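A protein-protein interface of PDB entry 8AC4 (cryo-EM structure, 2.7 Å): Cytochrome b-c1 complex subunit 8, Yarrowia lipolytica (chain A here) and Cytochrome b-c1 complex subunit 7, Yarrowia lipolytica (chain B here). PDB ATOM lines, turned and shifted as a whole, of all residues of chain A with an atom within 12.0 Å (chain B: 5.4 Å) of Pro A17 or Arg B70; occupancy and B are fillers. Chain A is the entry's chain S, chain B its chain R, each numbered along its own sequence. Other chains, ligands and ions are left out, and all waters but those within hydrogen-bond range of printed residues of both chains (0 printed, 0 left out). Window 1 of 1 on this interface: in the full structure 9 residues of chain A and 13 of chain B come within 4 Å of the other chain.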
ATOM      1  N   TYR A   7       5.882  15.970 -23.367  1.00  0.00           N
ATOM      2  CA  TYR A   7       4.410  15.468 -23.301  1.00  0.00           C
ATOM      3  C   TYR A   7       4.266  13.974 -23.606  1.00  0.00           C
ATOM      4  O   TYR A   7       3.209  13.364 -23.388  1.00  0.00           O
ATOM      5  CB  TYR A   7       3.472  16.242 -24.238  1.00  0.00           C
ATOM      6  CG  TYR A   7       3.138  17.643 -23.789  1.00  0.00           C
ATOM      7  CD1 TYR A   7       2.453  17.883 -22.605  1.00  0.00           C
ATOM      8  CD2 TYR A   7       3.554  18.737 -24.534  1.00  0.00           C
ATOM      9  CE1 TYR A   7       2.190  19.175 -22.170  1.00  0.00           C
ATOM     10  CE2 TYR A   7       3.289  20.033 -24.119  1.00  0.00           C
ATOM     11  CZ  TYR A   7       2.603  20.255 -22.935  1.00  0.00           C
ATOM     12  OH  TYR A   7       2.338  21.535 -22.532  1.00  0.00           O
ATOM     13  N   MET A   8       5.304  13.384 -24.185  1.00  0.00           N
ATOM     14  CA  MET A   8       5.361  11.939 -24.244  1.00  0.00           C
ATOM     15  C   MET A   8       6.691  11.509 -23.649  1.00  0.00           C
ATOM     16  O   MET A   8       7.721  12.118 -23.939  1.00  0.00           O
ATOM     17  CB  MET A   8       5.238  11.444 -25.680  1.00  0.00           C
ATOM     18  CG  MET A   8       5.239   9.940 -25.739  1.00  0.00           C
ATOM     19  SD  MET A   8       5.277   9.317 -27.414  1.00  0.00           S
ATOM     20  CE  MET A   8       6.916   9.803 -27.956  1.00  0.00           C
ATOM     21  N   GLY A   9       6.670  10.462 -22.821  1.00  0.00           N
ATOM     22  CA  GLY A   9       7.936   9.970 -22.322  1.00  0.00           C
ATOM     23  C   GLY A   9       8.421   8.791 -23.152  1.00  0.00           C
ATOM     24  O   GLY A   9       8.545   8.859 -24.375  1.00  0.00           O
ATOM     25  N   TRP A  10       8.705   7.705 -22.448  1.00  0.00           N
ATOM     26  CA  TRP A  10       9.197   6.500 -23.074  1.00  0.00           C
ATOM     27  C   TRP A  10       8.720   5.339 -22.220  1.00  0.00           C
ATOM     28  O   TRP A  10       8.130   5.558 -21.171  1.00  0.00           O
ATOM     29  CB  TRP A  10      10.720   6.539 -23.187  1.00  0.00           C
ATOM     30  CG  TRP A  10      11.210   5.644 -24.282  1.00  0.00           C
ATOM     31  CD1 TRP A  10      11.822   4.427 -24.161  1.00  0.00           C
ATOM     32  CD2 TRP A  10      11.057   5.884 -25.694  1.00  0.00           C
ATOM     33  NE1 TRP A  10      12.081   3.904 -25.404  1.00  0.00           N
ATOM     34  CE2 TRP A  10      11.625   4.775 -26.365  1.00  0.00           C
ATOM     35  CE3 TRP A  10      10.494   6.928 -26.447  1.00  0.00           C
ATOM     36  CZ2 TRP A  10      11.661   4.695 -27.761  1.00  0.00           C
ATOM     37  CZ3 TRP A  10      10.545   6.853 -27.825  1.00  0.00           C
ATOM     38  CH2 TRP A  10      11.117   5.749 -28.472  1.00  0.00           C
ATOM     39  N   GLY A  12       8.030   2.841 -19.574  1.00  0.00           N
ATOM     40  CA  GLY A  12       8.411   2.941 -18.183  1.00  0.00           C
ATOM     41  C   GLY A  12       8.044   4.292 -17.583  1.00  0.00           C
ATOM     42  O   GLY A  12       7.734   4.355 -16.397  1.00  0.00           O
ATOM     43  N   HIS A  13       8.069   5.357 -18.391  1.00  0.00           N
ATOM     44  CA  HIS A  13       7.715   6.674 -17.890  1.00  0.00           C
ATOM     45  C   HIS A  13       6.997   7.456 -18.985  1.00  0.00           C
ATOM     46  O   HIS A  13       7.405   8.556 -19.356  1.00  0.00           O
ATOM     47  CB  HIS A  13       8.966   7.358 -17.313  1.00  0.00           C
ATOM     48  CG  HIS A  13      10.047   7.522 -18.326  1.00  0.00           C
ATOM     49  ND1 HIS A  13      10.849   6.471 -18.729  1.00  0.00           N
ATOM     50  CD2 HIS A  13      10.434   8.600 -19.043  1.00  0.00           C
ATOM     51  CE1 HIS A  13      11.697   6.897 -19.642  1.00  0.00           C
ATOM     52  NE2 HIS A  13      11.457   8.201 -19.861  1.00  0.00           N
ATOM     53  N   MET A  14       5.907   6.881 -19.489  1.00  0.00           N
ATOM     54  CA  MET A  14       5.269   7.400 -20.684  1.00  0.00           C
ATOM     55  C   MET A  14       4.569   8.727 -20.397  1.00  0.00           C
ATOM     56  O   MET A  14       4.428   9.542 -21.298  1.00  0.00           O
ATOM     57  CB  MET A  14       4.238   6.408 -21.222  1.00  0.00           C
ATOM     58  CG  MET A  14       3.849   6.665 -22.663  1.00  0.00           C
ATOM     59  SD  MET A  14       5.221   6.272 -23.775  1.00  0.00           S
ATOM     60  CE  MET A  14       5.384   4.521 -23.434  1.00  0.00           C
ATOM     61  N   GLY A  15       4.146   8.954 -19.154  1.00  0.00           N
ATOM     62  CA  GLY A  15       3.448  10.189 -18.835  1.00  0.00           C
ATOM     63  C   GLY A  15       1.947   9.970 -18.662  1.00  0.00           C
ATOM     64  O   GLY A  15       1.164  10.922 -18.673  1.00  0.00           O
ATOM     65  N   SER A  16       1.559   8.709 -18.460  1.00  0.00           N
ATOM     66  CA  SER A  16       0.212   8.367 -18.041  1.00  0.00           C
ATOM     67  C   SER A  16      -0.033   8.910 -16.634  1.00  0.00           C
ATOM     68  O   SER A  16       0.883   8.965 -15.810  1.00  0.00           O
ATOM     69  CB  SER A  16       0.032   6.871 -18.098  1.00  0.00           C
ATOM     70  OG  SER A  16      -1.219   6.463 -17.563  1.00  0.00           O
ATOM     71  N   PRO A  17      -1.274   9.322 -16.294  1.00  0.00           N
ATOM     72  CA  PRO A  17      -1.645   9.476 -14.888  1.00  0.00           C
ATOM     73  C   PRO A  17      -1.496   8.089 -14.276  1.00  0.00           C
ATOM     74  O   PRO A  17      -1.532   7.099 -14.996  1.00  0.00           O
ATOM     75  CB  PRO A  17      -3.126   9.820 -14.965  1.00  0.00           C
ATOM     76  CG  PRO A  17      -3.282  10.445 -16.325  1.00  0.00           C
ATOM     77  CD  PRO A  17      -2.366   9.648 -17.223  1.00  0.00           C
ATOM     78  N   PRO A  18      -1.286   7.952 -12.952  1.00  0.00           N
ATOM     79  CA  PRO A  18      -1.132   6.626 -12.349  1.00  0.00           C
ATOM     80  C   PRO A  18      -2.320   5.730 -12.681  1.00  0.00           C
ATOM     81  O   PRO A  18      -3.468   6.161 -12.617  1.00  0.00           O
ATOM     82  CB  PRO A  18      -1.114   6.948 -10.855  1.00  0.00           C
ATOM     83  CG  PRO A  18      -0.534   8.338 -10.808  1.00  0.00           C
ATOM     84  CD  PRO A  18      -1.180   9.047 -11.976  1.00  0.00           C
ATOM     85  N   GLN A  19      -2.021   4.501 -13.094  1.00  0.00           N
ATOM     86  CA  GLN A  19      -3.064   3.541 -13.395  1.00  0.00           C
ATOM     87  C   GLN A  19      -3.154   2.561 -12.242  1.00  0.00           C
ATOM     88  O   GLN A  19      -2.139   2.142 -11.695  1.00  0.00           O
ATOM     89  CB  GLN A  19      -2.728   2.781 -14.663  1.00  0.00           C
ATOM     90  CG  GLN A  19      -2.456   3.720 -15.809  1.00  0.00           C
ATOM     91  CD  GLN A  19      -2.491   2.990 -17.122  1.00  0.00           C
ATOM     92  OE1 GLN A  19      -2.890   1.825 -17.202  1.00  0.00           O
ATOM     93  NE2 GLN A  19      -2.062   3.685 -18.165  1.00  0.00           N
ATOM     94  N   LYS A  20      -4.384   2.232 -11.864  1.00  0.00           N
ATOM     95  CA  LYS A  20      -4.616   1.255 -10.826  1.00  0.00           C
ATOM     96  C   LYS A  20      -6.003   0.697 -11.070  1.00  0.00           C
ATOM     97  O   LYS A  20      -6.888   1.422 -11.495  1.00  0.00           O
ATOM     98  CB  LYS A  20      -4.521   1.935  -9.460  1.00  0.00           C
ATOM     99  CG  LYS A  20      -4.626   0.997  -8.274  1.00  0.00           C
ATOM    100  CD  LYS A  20      -4.086   1.610  -7.007  1.00  0.00           C
ATOM    101  CE  LYS A  20      -4.446   0.808  -5.775  1.00  0.00           C
ATOM    102  NZ  LYS A  20      -4.246   1.599  -4.537  1.00  0.00           N
ATOM    103  N   GLY A  21      -6.176  -0.604 -10.855  1.00  0.00           N
ATOM    104  CA  GLY A  21      -7.513  -1.164 -10.870  1.00  0.00           C
ATOM    105  C   GLY A  21      -7.960  -1.697 -12.228  1.00  0.00           C
ATOM    106  O   GLY A  21      -9.032  -2.288 -12.308  1.00  0.00           O
ATOM    107  N   ILE A  22      -7.149  -1.563 -13.281  1.00  0.00           N
ATOM    108  CA  ILE A  22      -7.563  -2.143 -14.550  1.00  0.00           C
ATOM    109  C   ILE A  22      -6.828  -3.460 -14.772  1.00  0.00           C
ATOM    110  O   ILE A  22      -5.601  -3.477 -14.760  1.00  0.00           O
ATOM    111  CB  ILE A  22      -7.289  -1.161 -15.698  1.00  0.00           C
ATOM    112  CG1 ILE A  22      -7.925   0.208 -15.449  1.00  0.00           C
ATOM    113  CG2 ILE A  22      -7.730  -1.759 -17.025  1.00  0.00           C
ATOM    114  CD1 ILE A  22      -7.338   1.314 -16.305  1.00  0.00           C
ATOM    115  N   ASP B  46     -13.527  14.422 -20.829  1.00  0.00           N
ATOM    116  CA  ASP B  46     -12.442  13.562 -21.278  1.00  0.00           C
ATOM    117  C   ASP B  46     -11.905  14.017 -22.635  1.00  0.00           C
ATOM    118  O   ASP B  46     -10.791  13.652 -23.005  1.00  0.00           O
ATOM    119  CB  ASP B  46     -12.847  12.094 -21.375  1.00  0.00           C
ATOM    120  CG  ASP B  46     -13.453  11.509 -20.112  1.00  0.00           C
ATOM    121  OD1 ASP B  46     -13.003  11.880 -19.013  1.00  0.00           O
ATOM    122  OD2 ASP B  46     -14.363  10.666 -20.237  1.00  0.00           O
ATOM    123  N   GLU B  50      -5.232  18.180 -23.455  1.00  0.00           N
ATOM    124  CA  GLU B  50      -4.566  18.193 -22.167  1.00  0.00           C
ATOM    125  C   GLU B  50      -3.086  18.550 -22.276  1.00  0.00           C
ATOM    126  O   GLU B  50      -2.423  18.654 -21.251  1.00  0.00           O
ATOM    127  CB  GLU B  50      -4.744  16.841 -21.489  1.00  0.00           C
ATOM    128  CG  GLU B  50      -3.865  15.795 -22.142  1.00  0.00           C
ATOM    129  CD  GLU B  50      -3.648  14.537 -21.324  1.00  0.00           C
ATOM    130  OE1 GLU B  50      -2.514  14.350 -20.831  1.00  0.00           O
ATOM    131  OE2 GLU B  50      -4.607  13.746 -21.176  1.00  0.00           O
ATOM    132  N   LEU B  59      -5.013  18.333 -14.202  1.00  0.00           N
ATOM    133  CA  LEU B  59      -5.200  16.897 -14.087  1.00  0.00           C
ATOM    134  C   LEU B  59      -4.521  16.348 -12.839  1.00  0.00           C
ATOM    135  O   LEU B  59      -5.024  15.396 -12.252  1.00  0.00           O
ATOM    136  CB  LEU B  59      -4.721  16.199 -15.359  1.00  0.00           C
ATOM    137  CG  LEU B  59      -5.674  16.355 -16.543  1.00  0.00           C
ATOM    138  CD1 LEU B  59      -5.005  15.951 -17.841  1.00  0.00           C
ATOM    139  CD2 LEU B  59      -6.953  15.570 -16.323  1.00  0.00           C
ATOM    140  N   LEU B  62      -6.797  16.508  -9.835  1.00  0.00           N
ATOM    141  CA  LEU B  62      -7.962  15.647  -9.701  1.00  0.00           C
ATOM    142  C   LEU B  62      -7.813  14.746  -8.484  1.00  0.00           C
ATOM    143  O   LEU B  62      -6.723  14.231  -8.224  1.00  0.00           O
ATOM    144  CB  LEU B  62      -8.053  14.746 -10.927  1.00  0.00           C
ATOM    145  CG  LEU B  62      -8.752  15.329 -12.140  1.00  0.00           C
ATOM    146  CD1 LEU B  62      -8.843  14.253 -13.207  1.00  0.00           C
ATOM    147  CD2 LEU B  62     -10.140  15.808 -11.753  1.00  0.00           C
ATOM    148  N   THR B  65      -9.446   8.967  -7.134  1.00  0.00           N
ATOM    149  CA  THR B  65     -10.552   8.186  -7.663  1.00  0.00           C
ATOM    150  C   THR B  65     -10.982   8.679  -9.045  1.00  0.00           C
ATOM    151  O   THR B  65     -11.120   7.879  -9.965  1.00  0.00           O
ATOM    152  CB  THR B  65     -11.731   8.243  -6.686  1.00  0.00           C
ATOM    153  OG1 THR B  65     -11.261   7.699  -5.453  1.00  0.00           O
ATOM    154  CG2 THR B  65     -12.959   7.489  -7.142  1.00  0.00           C
ATOM    155  N   GLU B  66     -11.241   9.984  -9.165  1.00  0.00           N
ATOM    156  CA  GLU B  66     -11.649  10.579 -10.428  1.00  0.00           C
ATOM    157  C   GLU B  66     -10.565  10.345 -11.476  1.00  0.00           C
ATOM    158  O   GLU B  66     -10.847  10.086 -12.644  1.00  0.00           O
ATOM    159  CB  GLU B  66     -11.900  12.080 -10.273  1.00  0.00           C
ATOM    160  CG  GLU B  66     -13.147  12.418  -9.481  1.00  0.00           C
ATOM    161  CD  GLU B  66     -14.444  12.549 -10.268  1.00  0.00           C
ATOM    162  OE1 GLU B  66     -15.306  13.347  -9.840  1.00  0.00           O
ATOM    163  OE2 GLU B  66     -14.604  11.852 -11.294  1.00  0.00           O
ATOM    164  N   SER B  67      -9.316  10.443 -11.038  1.00  0.00           N
ATOM    165  CA  SER B  67      -8.228  10.273 -11.968  1.00  0.00           C
ATOM    166  C   SER B  67      -8.165   8.830 -12.474  1.00  0.00           C
ATOM    167  O   SER B  67      -7.943   8.620 -13.665  1.00  0.00           O
ATOM    168  CB  SER B  67      -6.968  10.698 -11.337  1.00  0.00           C
ATOM    169  OG  SER B  67      -5.907  10.602 -12.270  1.00  0.00           O
ATOM    170  N   TYR B  68      -8.350   7.856 -11.572  1.00  0.00           N
ATOM    171  CA  TYR B  68      -8.270   6.459 -11.951  1.00  0.00           C
ATOM    172  C   TYR B  68      -9.389   6.126 -12.916  1.00  0.00           C
ATOM    173  O   TYR B  68      -9.174   5.342 -13.834  1.00  0.00           O
ATOM    174  CB  TYR B  68      -8.412   5.514 -10.763  1.00  0.00           C
ATOM    175  CG  TYR B  68      -7.219   5.526  -9.858  1.00  0.00           C
ATOM    176  CD1 TYR B  68      -5.927   5.508 -10.368  1.00  0.00           C
ATOM    177  CD2 TYR B  68      -7.386   5.560  -8.485  1.00  0.00           C
ATOM    178  CE1 TYR B  68      -4.825   5.522  -9.529  1.00  0.00           C
ATOM    179  CE2 TYR B  68      -6.291   5.559  -7.634  1.00  0.00           C
ATOM    180  CZ  TYR B  68      -5.009   5.547  -8.157  1.00  0.00           C
ATOM    181  OH  TYR B  68      -3.930   5.556  -7.320  1.00  0.00           O
ATOM    182  N   ASP B  69     -10.557   6.730 -12.692  1.00  0.00           N
ATOM    183  CA  ASP B  69     -11.698   6.424 -13.528  1.00  0.00           C
ATOM    184  C   ASP B  69     -11.490   7.007 -14.920  1.00  0.00           C
ATOM    185  O   ASP B  69     -11.929   6.436 -15.915  1.00  0.00           O
ATOM    186  CB  ASP B  69     -12.978   6.987 -12.930  1.00  0.00           C
ATOM    187  CG  ASP B  69     -13.446   6.279 -11.670  1.00  0.00           C
ATOM    188  OD1 ASP B  69     -12.843   5.244 -11.299  1.00  0.00           O
ATOM    189  OD2 ASP B  69     -14.424   6.768 -11.060  1.00  0.00           O
ATOM    190  N   ARG B  70     -10.871   8.184 -14.983  1.00  0.00           N
ATOM    191  CA  ARG B  70     -10.634   8.800 -16.272  1.00  0.00           C
ATOM    192  C   ARG B  70      -9.682   7.920 -17.078  1.00  0.00           C
ATOM    193  O   ARG B  70      -9.910   7.696 -18.259  1.00  0.00           O
ATOM    194  CB  ARG B  70     -10.107  10.212 -16.051  1.00  0.00           C
ATOM    195  CG  ARG B  70      -9.585  10.898 -17.303  1.00  0.00           C
ATOM    196  CD  ARG B  70      -9.088  12.298 -17.009  1.00  0.00           C
ATOM    197  NE  ARG B  70      -8.540  12.908 -18.211  1.00  0.00           N
ATOM    198  CZ  ARG B  70      -7.285  12.745 -18.607  1.00  0.00           C
ATOM    199  NH1 ARG B  70      -6.855  13.340 -19.709  1.00  0.00           N
ATOM    200  NH2 ARG B  70      -6.466  11.997 -17.884  1.00  0.00           N
ATOM    201  N   VAL B  71      -8.637   7.401 -16.435  1.00  0.00           N
ATOM    202  CA  VAL B  71      -7.694   6.558 -17.147  1.00  0.00           C
ATOM    203  C   VAL B  71      -8.428   5.345 -17.703  1.00  0.00           C
ATOM    204  O   VAL B  71      -8.263   4.992 -18.862  1.00  0.00           O
ATOM    205  CB  VAL B  71      -6.519   6.143 -16.254  1.00  0.00           C
ATOM    206  CG1 VAL B  71      -5.823   4.903 -16.787  1.00  0.00           C
ATOM    207  CG2 VAL B  71      -5.527   7.279 -16.091  1.00  0.00           C
ATOM    208  N   TYR B  72      -9.309   4.745 -16.918  1.00  0.00           N
ATOM    209  CA  TYR B  72     -10.056   3.641 -17.478  1.00  0.00           C
ATOM    210  C   TYR B  72     -10.937   4.060 -18.656  1.00  0.00           C
ATOM    211  O   TYR B  72     -10.966   3.360 -19.658  1.00  0.00           O
ATOM    212  CB  TYR B  72     -10.872   2.957 -16.398  1.00  0.00           C
ATOM    213  CG  TYR B  72     -11.771   1.904 -16.965  1.00  0.00           C
ATOM    214  CD1 TYR B  72     -11.235   0.773 -17.566  1.00  0.00           C
ATOM    215  CD2 TYR B  72     -13.149   2.056 -16.949  1.00  0.00           C
ATOM    216  CE1 TYR B  72     -12.053  -0.197 -18.122  1.00  0.00           C
ATOM    217  CE2 TYR B  72     -13.981   1.078 -17.472  1.00  0.00           C
ATOM    218  CZ  TYR B  72     -13.430  -0.051 -18.064  1.00  0.00           C
ATOM    219  OH  TYR B  72     -14.230  -1.024 -18.595  1.00  0.00           O
ATOM    220  N   ARG B  73     -11.673   5.169 -18.558  1.00  0.00           N
ATOM    221  CA  ARG B  73     -12.485   5.584 -19.695  1.00  0.00           C
ATOM    222  C   ARG B  73     -11.636   5.813 -20.949  1.00  0.00           C
ATOM    223  O   ARG B  73     -12.085   5.498 -22.042  1.00  0.00           O
ATOM    224  CB  ARG B  73     -13.309   6.830 -19.393  1.00  0.00           C
ATOM    225  CG  ARG B  73     -14.511   6.569 -18.502  1.00  0.00           C
ATOM    226  CD  ARG B  73     -15.437   7.773 -18.387  1.00  0.00           C
ATOM    227  NE  ARG B  73     -14.734   9.011 -18.084  1.00  0.00           N
ATOM    228  CZ  ARG B  73     -14.360   9.404 -16.875  1.00  0.00           C
ATOM    229  NH1 ARG B  73     -13.707  10.544 -16.743  1.00  0.00           N
ATOM    230  NH2 ARG B  73     -14.639   8.665 -15.813  1.00  0.00           N
ATOM    231  N   LEU B  74     -10.433   6.377 -20.810  1.00  0.00           N
ATOM    232  CA  LEU B  74      -9.629   6.614 -21.993  1.00  0.00           C
ATOM    233  C   LEU B  74      -9.170   5.293 -22.597  1.00  0.00           C
ATOM    234  O   LEU B  74      -9.171   5.155 -23.820  1.00  0.00           O
ATOM    235  CB  LEU B  74      -8.432   7.503 -21.667  1.00  0.00           C
ATOM    236  CG  LEU B  74      -8.760   8.915 -21.184  1.00  0.00           C
ATOM    237  CD1 LEU B  74      -7.484   9.685 -20.908  1.00  0.00           C
ATOM    238  CD2 LEU B  74      -9.631   9.664 -22.182  1.00  0.00           C
ATOM    239  N   ILE B  75      -8.834   4.324 -21.741  1.00  0.00           N
ATOM    240  CA  ILE B  75      -8.321   3.072 -22.258  1.00  0.00           C
ATOM    241  C   ILE B  75      -9.456   2.311 -22.915  1.00  0.00           C
ATOM    242  O   ILE B  75      -9.289   1.808 -24.014  1.00  0.00           O
ATOM    243  CB  ILE B  75      -7.646   2.253 -21.163  1.00  0.00           C
ATOM    244  CG1 ILE B  75      -6.259   2.828 -20.915  1.00  0.00           C
ATOM    245  CG2 ILE B  75      -7.579   0.789 -21.551  1.00  0.00           C
ATOM    246  CD1 ILE B  75      -5.717   2.478 -19.563  1.00  0.00           C
ATOM    247  N   TYR B 101     -16.371  16.911 -14.296  1.00  0.00           N
ATOM    248  CA  TYR B 101     -15.539  16.600 -13.145  1.00  0.00           C
ATOM    249  C   TYR B 101     -14.289  17.474 -13.200  1.00  0.00           C
ATOM    250  O   TYR B 101     -13.686  17.744 -12.179  1.00  0.00           O
ATOM    251  CB  TYR B 101     -15.205  15.102 -13.085  1.00  0.00           C
ATOM    252  CG  TYR B 101     -14.367  14.665 -14.255  1.00  0.00           C
ATOM    253  CD1 TYR B 101     -12.982  14.744 -14.194  1.00  0.00           C
ATOM    254  CD2 TYR B 101     -14.953  14.268 -15.452  1.00  0.00           C
ATOM    255  CE1 TYR B 101     -12.196  14.417 -15.290  1.00  0.00           C
ATOM    256  CE2 TYR B 101     -14.177  13.944 -16.557  1.00  0.00           C
ATOM    257  CZ  TYR B 101     -12.792  14.009 -16.475  1.00  0.00           C
ATOM    258  OH  TYR B 101     -12.023  13.700 -17.567  1.00  0.00           O
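The side-chain carboxylate (OE2) of Glu B50 is in salt-bridge range of the guanidinium group (NH1) of Arg B70. The side-chain hydroxyl of Ser A16 sits at hydrogen-bond distance from the side-chain amide nitrogen of Gln A19.
Among the printed residues, merely in contact across the chains: Pro A18 with Tyr B68 (3.4 Å), Lys A20 with Tyr B68 (3.6 Å), Pro A17 with Val B71 (3.7 Å), Gln A19 with Val B71 (3.7 Å), Gln A19 with Ile B75 (3.7 Å), Ile A22 with Tyr B72 (3.8 Å), Ile A22 with Ile B75 (3.8 Å), Pro A17 with Arg B70 (3.9 Å), Ile A22 with Val B71 (3.9 Å) and Pro A17 with Ser B67 (3.95 Å).
Of the 16 printed residues of chain B, 6 touch a printed residue of chain A. Hydrophobic or aromatic side chains of chain B that line the printed part of chain A: Tyr B68, Val B71, Tyr B72 and Ile B75. Hydrophobic or aromatic side chains of chain A that line the printed part of chain B: Pro A17 and Ile A22. Among the printed residues, 10 pairs touch across the chains.
Gly A15 touches none of the printed residues of chain B. Of chain B, only Ser B67, Arg B70 and Val B71 come within 4 Å of Pro A17. Printed residues of chain B within 4 Å of Pro A18: Tyr B68. Of the printed residues of chain B, Ile A22 touches Val B71, Tyr B72 and Ile B75. No residue of chain A comes within 4 Å of Asp B46. No residue of chain A comes within 4 Å of Glu B50. Of chain A, only Pro A17 comes within 4 Å of Arg B70. Printed residues of chain A within 4 Å of Tyr B72: Ile A22. No residue of chain A comes within 4 Å of Arg B73. Of the printed residues of chain A, Ile B75 touches Gln A19 (3.7 Å) and Ile A22 (3.8 Å). The nearest printed residue of chain B that does not touch Pro A17 is Glu B50 (5.9 Å). The nearest residue of chain A that does not touch Arg B70 is Ile A22 (7.1 Å).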
